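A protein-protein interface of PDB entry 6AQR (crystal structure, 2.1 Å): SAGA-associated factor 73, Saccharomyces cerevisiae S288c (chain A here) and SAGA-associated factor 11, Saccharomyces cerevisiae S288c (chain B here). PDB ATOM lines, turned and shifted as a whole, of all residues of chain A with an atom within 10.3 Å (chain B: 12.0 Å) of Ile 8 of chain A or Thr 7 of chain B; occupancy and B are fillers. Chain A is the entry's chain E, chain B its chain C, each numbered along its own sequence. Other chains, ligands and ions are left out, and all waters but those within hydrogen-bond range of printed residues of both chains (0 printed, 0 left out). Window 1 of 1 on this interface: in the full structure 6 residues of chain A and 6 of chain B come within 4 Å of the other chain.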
ATOM      1  N   GLY A   4      12.929  14.942 -21.259  1.00  0.00           N
ATOM      2  CA  GLY A   4      11.534  15.137 -21.811  1.00  0.00           C
ATOM      3  C   GLY A   4      10.656  16.112 -21.000  1.00  0.00           C
ATOM      4  O   GLY A   4       9.928  16.952 -21.562  1.00  0.00           O
ATOM      5  N   ASP A   5      10.717  15.981 -19.667  1.00  0.00           N
ATOM      6  CA  ASP A   5      10.086  16.912 -18.685  1.00  0.00           C
ATOM      7  C   ASP A   5      10.806  18.268 -18.534  1.00  0.00           C
ATOM      8  O   ASP A   5      10.325  19.141 -17.816  1.00  0.00           O
ATOM      9  CB  ASP A   5       9.983  16.251 -17.308  1.00  0.00           C
ATOM     10  CG  ASP A   5       8.949  15.122 -17.251  1.00  0.00           C
ATOM     11  OD1 ASP A   5       7.996  15.065 -18.088  1.00  0.00           O
ATOM     12  OD2 ASP A   5       9.103  14.285 -16.326  1.00  0.00           O
ATOM     13  N   ALA A   6      11.942  18.434 -19.225  1.00  0.00           N
ATOM     14  CA  ALA A   6      12.687  19.697 -19.327  1.00  0.00           C
ATOM     15  C   ALA A   6      11.857  20.925 -19.794  1.00  0.00           C
ATOM     16  O   ALA A   6      11.121  20.854 -20.795  1.00  0.00           O
ATOM     17  CB  ALA A   6      13.881  19.488 -20.238  1.00  0.00           C
ATOM     18  N   GLU A   7      11.982  22.035 -19.056  1.00  0.00           N
ATOM     19  CA  GLU A   7      11.251  23.267 -19.303  1.00  0.00           C
ATOM     20  C   GLU A   7      11.902  24.138 -20.409  1.00  0.00           C
ATOM     21  O   GLU A   7      13.141  24.188 -20.537  1.00  0.00           O
ATOM     22  CB  GLU A   7      11.143  24.046 -17.979  1.00  0.00           C
ATOM     23  CG  GLU A   7      10.729  25.505 -18.114  1.00  0.00           C
ATOM     24  CD  GLU A   7      10.144  26.104 -16.839  1.00  0.00           C
ATOM     25  OE1 GLU A   7       9.191  26.929 -16.974  1.00  0.00           O
ATOM     26  OE2 GLU A   7      10.632  25.757 -15.720  1.00  0.00           O
ATOM     27  N   ILE A   8      11.033  24.827 -21.166  1.00  0.00           N
ATOM     28  CA  ILE A   8      11.372  25.709 -22.302  1.00  0.00           C
ATOM     29  C   ILE A   8      11.507  27.163 -21.866  1.00  0.00           C
ATOM     30  O   ILE A   8      10.518  27.796 -21.473  1.00  0.00           O
ATOM     31  CB  ILE A   8      10.334  25.598 -23.461  1.00  0.00           C
ATOM     32  CG1 ILE A   8      10.353  24.170 -24.034  1.00  0.00           C
ATOM     33  CG2 ILE A   8      10.585  26.650 -24.548  1.00  0.00           C
ATOM     34  CD1 ILE A   8       9.275  23.854 -25.043  1.00  0.00           C
ATOM     35  N   LYS A   9      12.736  27.681 -21.965  1.00  0.00           N
ATOM     36  CA  LYS A   9      13.052  29.068 -21.598  1.00  0.00           C
ATOM     37  C   LYS A   9      12.546  30.050 -22.669  1.00  0.00           C
ATOM     38  O   LYS A   9      11.895  31.061 -22.349  1.00  0.00           O
ATOM     39  CB  LYS A   9      14.560  29.240 -21.316  1.00  0.00           C
ATOM     40  CG  LYS A   9      15.171  28.181 -20.384  1.00  0.00           C
ATOM     41  CD  LYS A   9      16.512  28.596 -19.776  1.00  0.00           C
ATOM     42  CE  LYS A   9      16.316  29.276 -18.403  1.00  0.00           C
ATOM     43  NZ  LYS A   9      17.577  29.482 -17.614  1.00  0.00           N
ATOM     44  N   GLY A  10      12.833  29.717 -23.934  1.00  0.00           N
ATOM     45  CA  GLY A  10      12.415  30.489 -25.121  1.00  0.00           C
ATOM     46  C   GLY A  10      12.991  29.858 -26.382  1.00  0.00           C
ATOM     47  O   GLY A  10      13.667  28.820 -26.323  1.00  0.00           O
ATOM     48  N   ILE A  11      12.735  30.488 -27.524  1.00  0.00           N
ATOM     49  CA  ILE A  11      13.292  30.029 -28.816  1.00  0.00           C
ATOM     50  C   ILE A  11      14.737  30.547 -28.917  1.00  0.00           C
ATOM     51  O   ILE A  11      14.969  31.701 -28.553  1.00  0.00           O
ATOM     52  CB  ILE A  11      12.388  30.520 -29.985  1.00  0.00           C
ATOM     53  CG1 ILE A  11      11.130  29.639 -30.078  1.00  0.00           C
ATOM     54  CG2 ILE A  11      13.106  30.492 -31.320  1.00  0.00           C
ATOM     55  CD1 ILE A  11       9.836  30.437 -30.321  1.00  0.00           C
ATOM     56  N   LYS A  12      15.690  29.719 -29.380  1.00  0.00           N
ATOM     57  CA  LYS A  12      17.083  30.167 -29.636  1.00  0.00           C
ATOM     58  C   LYS A  12      17.108  31.446 -30.459  1.00  0.00           C
ATOM     59  O   LYS A  12      16.400  31.512 -31.464  1.00  0.00           O
ATOM     60  CB  LYS A  12      17.917  29.091 -30.325  1.00  0.00           C
ATOM     61  CG  LYS A  12      18.132  27.889 -29.439  1.00  0.00           C
ATOM     62  CD  LYS A  12      18.999  26.806 -30.057  1.00  0.00           C
ATOM     63  CE  LYS A  12      19.190  25.737 -29.000  1.00  0.00           C
ATOM     64  NZ  LYS A  12      19.633  24.419 -29.510  1.00  0.00           N
ATOM     65  N   THR B   7       6.989  23.056 -21.326  1.00  0.00           N
ATOM     66  CA  THR B   7       7.906  21.872 -21.490  1.00  0.00           C
ATOM     67  C   THR B   7       8.054  21.323 -22.940  1.00  0.00           C
ATOM     68  O   THR B   7       7.184  21.512 -23.761  1.00  0.00           O
ATOM     69  CB  THR B   7       7.654  20.738 -20.437  1.00  0.00           C
ATOM     70  OG1 THR B   7       8.508  19.612 -20.695  1.00  0.00           O
ATOM     71  CG2 THR B   7       6.236  20.237 -20.402  1.00  0.00           C
ATOM     72  N   ILE B   8       9.171  20.653 -23.231  1.00  0.00           N
ATOM     73  CA  ILE B   8       9.352  19.849 -24.462  1.00  0.00           C
ATOM     74  C   ILE B   8       8.210  18.857 -24.749  1.00  0.00           C
ATOM     75  O   ILE B   8       7.669  18.893 -25.842  1.00  0.00           O
ATOM     76  CB  ILE B   8      10.706  19.093 -24.447  1.00  0.00           C
ATOM     77  CG1 ILE B   8      11.886  20.097 -24.397  1.00  0.00           C
ATOM     78  CG2 ILE B   8      10.831  18.076 -25.598  1.00  0.00           C
ATOM     79  CD1 ILE B   8      11.810  21.256 -25.367  1.00  0.00           C
ATOM     80  N   ASP B   9       7.865  17.989 -23.783  1.00  0.00           N
ATOM     81  CA  ASP B   9       6.655  17.143 -23.826  1.00  0.00           C
ATOM     82  C   ASP B   9       5.319  17.880 -23.931  1.00  0.00           C
ATOM     83  O   ASP B   9       4.435  17.424 -24.636  1.00  0.00           O
ATOM     84  CB  ASP B   9       6.580  16.218 -22.617  1.00  0.00           C
ATOM     85  CG  ASP B   9       7.517  15.072 -22.717  1.00  0.00           C
ATOM     86  OD1 ASP B   9       8.284  15.037 -23.703  1.00  0.00           O
ATOM     87  OD2 ASP B   9       7.507  14.201 -21.807  1.00  0.00           O
ATOM     88  N   SER B  10       5.165  18.985 -23.213  1.00  0.00           N
ATOM     89  CA  SER B  10       3.981  19.829 -23.321  1.00  0.00           C
ATOM     90  C   SER B  10       3.735  20.187 -24.797  1.00  0.00           C
ATOM     91  O   SER B  10       2.720  19.817 -25.382  1.00  0.00           O
ATOM     92  CB  SER B  10       4.187  21.119 -22.483  1.00  0.00           C
ATOM     93  OG  SER B  10       3.315  22.193 -22.857  1.00  0.00           O
ATOM     94  N   ILE B  11       4.683  20.932 -25.366  1.00  0.00           N
ATOM     95  CA  ILE B  11       4.591  21.414 -26.703  1.00  0.00           C
ATOM     96  C   ILE B  11       4.528  20.252 -27.732  1.00  0.00           C
ATOM     97  O   ILE B  11       3.655  20.267 -28.588  1.00  0.00           O
ATOM     98  CB  ILE B  11       5.617  22.522 -26.970  1.00  0.00           C
ATOM     99  CG1 ILE B  11       5.060  23.795 -26.344  1.00  0.00           C
ATOM    100  CG2 ILE B  11       5.771  22.742 -28.459  1.00  0.00           C
ATOM    101  CD1 ILE B  11       5.969  24.985 -26.476  1.00  0.00           C
ATOM    102  N   SER B  12       5.360  19.226 -27.577  1.00  0.00           N
ATOM    103  CA  SER B  12       5.273  18.073 -28.450  1.00  0.00           C
ATOM    104  C   SER B  12       3.852  17.498 -28.526  1.00  0.00           C
ATOM    105  O   SER B  12       3.382  17.216 -29.623  1.00  0.00           O
ATOM    106  CB  SER B  12       6.266  17.009 -28.057  1.00  0.00           C
ATOM    107  OG  SER B  12       7.579  17.513 -28.300  1.00  0.00           O
ATOM    108  N   ASN B  13       3.172  17.385 -27.380  1.00  0.00           N
ATOM    109  CA  ASN B  13       1.836  16.797 -27.307  1.00  0.00           C
ATOM    110  C   ASN B  13       0.870  17.691 -27.965  1.00  0.00           C
ATOM    111  O   ASN B  13      -0.041  17.211 -28.593  1.00  0.00           O
ATOM    112  CB  ASN B  13       1.332  16.596 -25.851  1.00  0.00           C
ATOM    113  CG  ASN B  13       1.997  15.446 -25.150  1.00  0.00           C
ATOM    114  OD1 ASN B  13       2.430  14.456 -25.765  1.00  0.00           O
ATOM    115  ND2 ASN B  13       2.073  15.559 -23.822  1.00  0.00           N
ATOM    116  N   GLY B  14       1.011  18.985 -27.744  1.00  0.00           N
ATOM    117  CA  GLY B  14       0.122  19.974 -28.370  1.00  0.00           C
ATOM    118  C   GLY B  14       0.224  19.899 -29.906  1.00  0.00           C
ATOM    119  O   GLY B  14      -0.771  20.055 -30.593  1.00  0.00           O
ATOM    120  N   ILE B  15       1.426  19.630 -30.444  1.00  0.00           N
ATOM    121  CA  ILE B  15       1.638  19.704 -31.864  1.00  0.00           C
ATOM    122  C   ILE B  15       0.998  18.440 -32.423  1.00  0.00           C
ATOM    123  O   ILE B  15       0.246  18.503 -33.397  1.00  0.00           O
ATOM    124  CB  ILE B  15       3.142  19.810 -32.228  1.00  0.00           C
ATOM    125  CG1 ILE B  15       3.633  21.236 -32.010  1.00  0.00           C
ATOM    126  CG2 ILE B  15       3.389  19.306 -33.668  1.00  0.00           C
ATOM    127  CD1 ILE B  15       5.113  21.318 -31.960  1.00  0.00           C
ATOM    128  N   LEU B  16       1.254  17.308 -31.784  1.00  0.00           N
ATOM    129  CA  LEU B  16       0.642  16.094 -32.205  1.00  0.00           C
ATOM    130  C   LEU B  16      -0.910  16.163 -32.135  1.00  0.00           C
ATOM    131  O   LEU B  16      -1.582  15.626 -33.010  1.00  0.00           O
ATOM    132  CB  LEU B  16       1.168  14.929 -31.407  1.00  0.00           C
ATOM    133  CG  LEU B  16       0.503  13.577 -31.574  1.00  0.00           C
ATOM    134  CD1 LEU B  16       0.710  13.015 -32.980  1.00  0.00           C
ATOM    135  CD2 LEU B  16       1.001  12.590 -30.528  1.00  0.00           C
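The backbone carbonyl oxygen (O) of Ala 6 of chain A sits at hydrogen-bond distance from the backbone NH (N) of Ile 8 of chain B. The backbone carbonyl oxygen of Gly 4 of chain A lies within hydrogen-bond range of the backbone NH of Asp 9 of chain B (3.2 Å). The side-chain hydroxyl (OG1) of Thr 7 of chain B sits at hydrogen-bond distance from the backbone carbonyl oxygen (O) of Ala 6 of chain A, 2.9 Å away. O of Gly 4 of chain A lies within hydrogen-bond range of OG1 of Thr 7 of chain B (3.1 Å). The side-chain hydroxyl (OG1) of Thr 7 of chain B lies close to the backbone carbonyl oxygen (O) of Asp 5 of chain A, at 3.4 Å.
The backbone carbonyl oxygen of Asp 9 of chain B is in hydrogen-bond range of the side-chain amide nitrogen of Asn 13 of chain B, at 3.1 Å. The backbone carbonyl oxygen of Ile 8 of chain B is in hydrogen-bond range of the side-chain hydroxyl of Ser 12 of chain B.
Gly 4 of chain A touches Ile 8 of chain B (O to CB, 3.7 Å). OD1 of Asp 5 of chain A touches OD2 of Asp 9 of chain B (3.8 Å). Thr 7 of chain B touches Ile 8 of chain A. Ile 8 of chain A touches Ile 8 of chain B (CG1 to CD1, 3.5 Å). Ile 11 of chain B touches Ile 8 of chain A (CD1 to CD1, 3.8 Å).
Ile 8 of chain A touches three residues of chain B. Of chain A, only Gly 4, Asp 5, Ala 6 and Ile 8 come within 4 Å of Thr 7 of chain B. Gly 4 of chain A touches just these residues of chain B: Thr 7 (3.1 Å), Ile 8 (3.7 Å) and Asp 9 (3.2 Å). Of the printed residues of chain B, Asp 5 of chain A touches Thr 7 (3.4 Å) and Asp 9 (3.8 Å). No residue of chain B comes within 4 Å of Glu 7 of chain A. No residue of chain B comes within 4 Å of Lys 9 of chain A. Gly 10 of chain A touches none of the printed residues of chain B. Of chain A, only Gly 4, Ala 6 and Ile 8 come within 4 Å of Ile 8 of chain B. Of chain A, only Gly 4 (3.2 Å) and Asp 5 (3.8 Å) come within 4 Å of Asp 9 of chain B. No residue of chain A comes within 4 Å of Ser 10 of chain B. Of chain A, only Ile 8 (3.8 Å) comes within 4 Å of Ile 11 of chain B. Ile 15 of chain B touches none of the printed residues of chain A.
Hydrophobic or aromatic side chains of chain B within 4 Å of the printed part of chain A: Ile 8 and Ile 11. Of the 9 printed residues of chain A, 4 touch a printed residue of chain B. Hydrophobic or aromatic side chains of chain A within 4 Å of the printed part of chain B: Ile 8.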
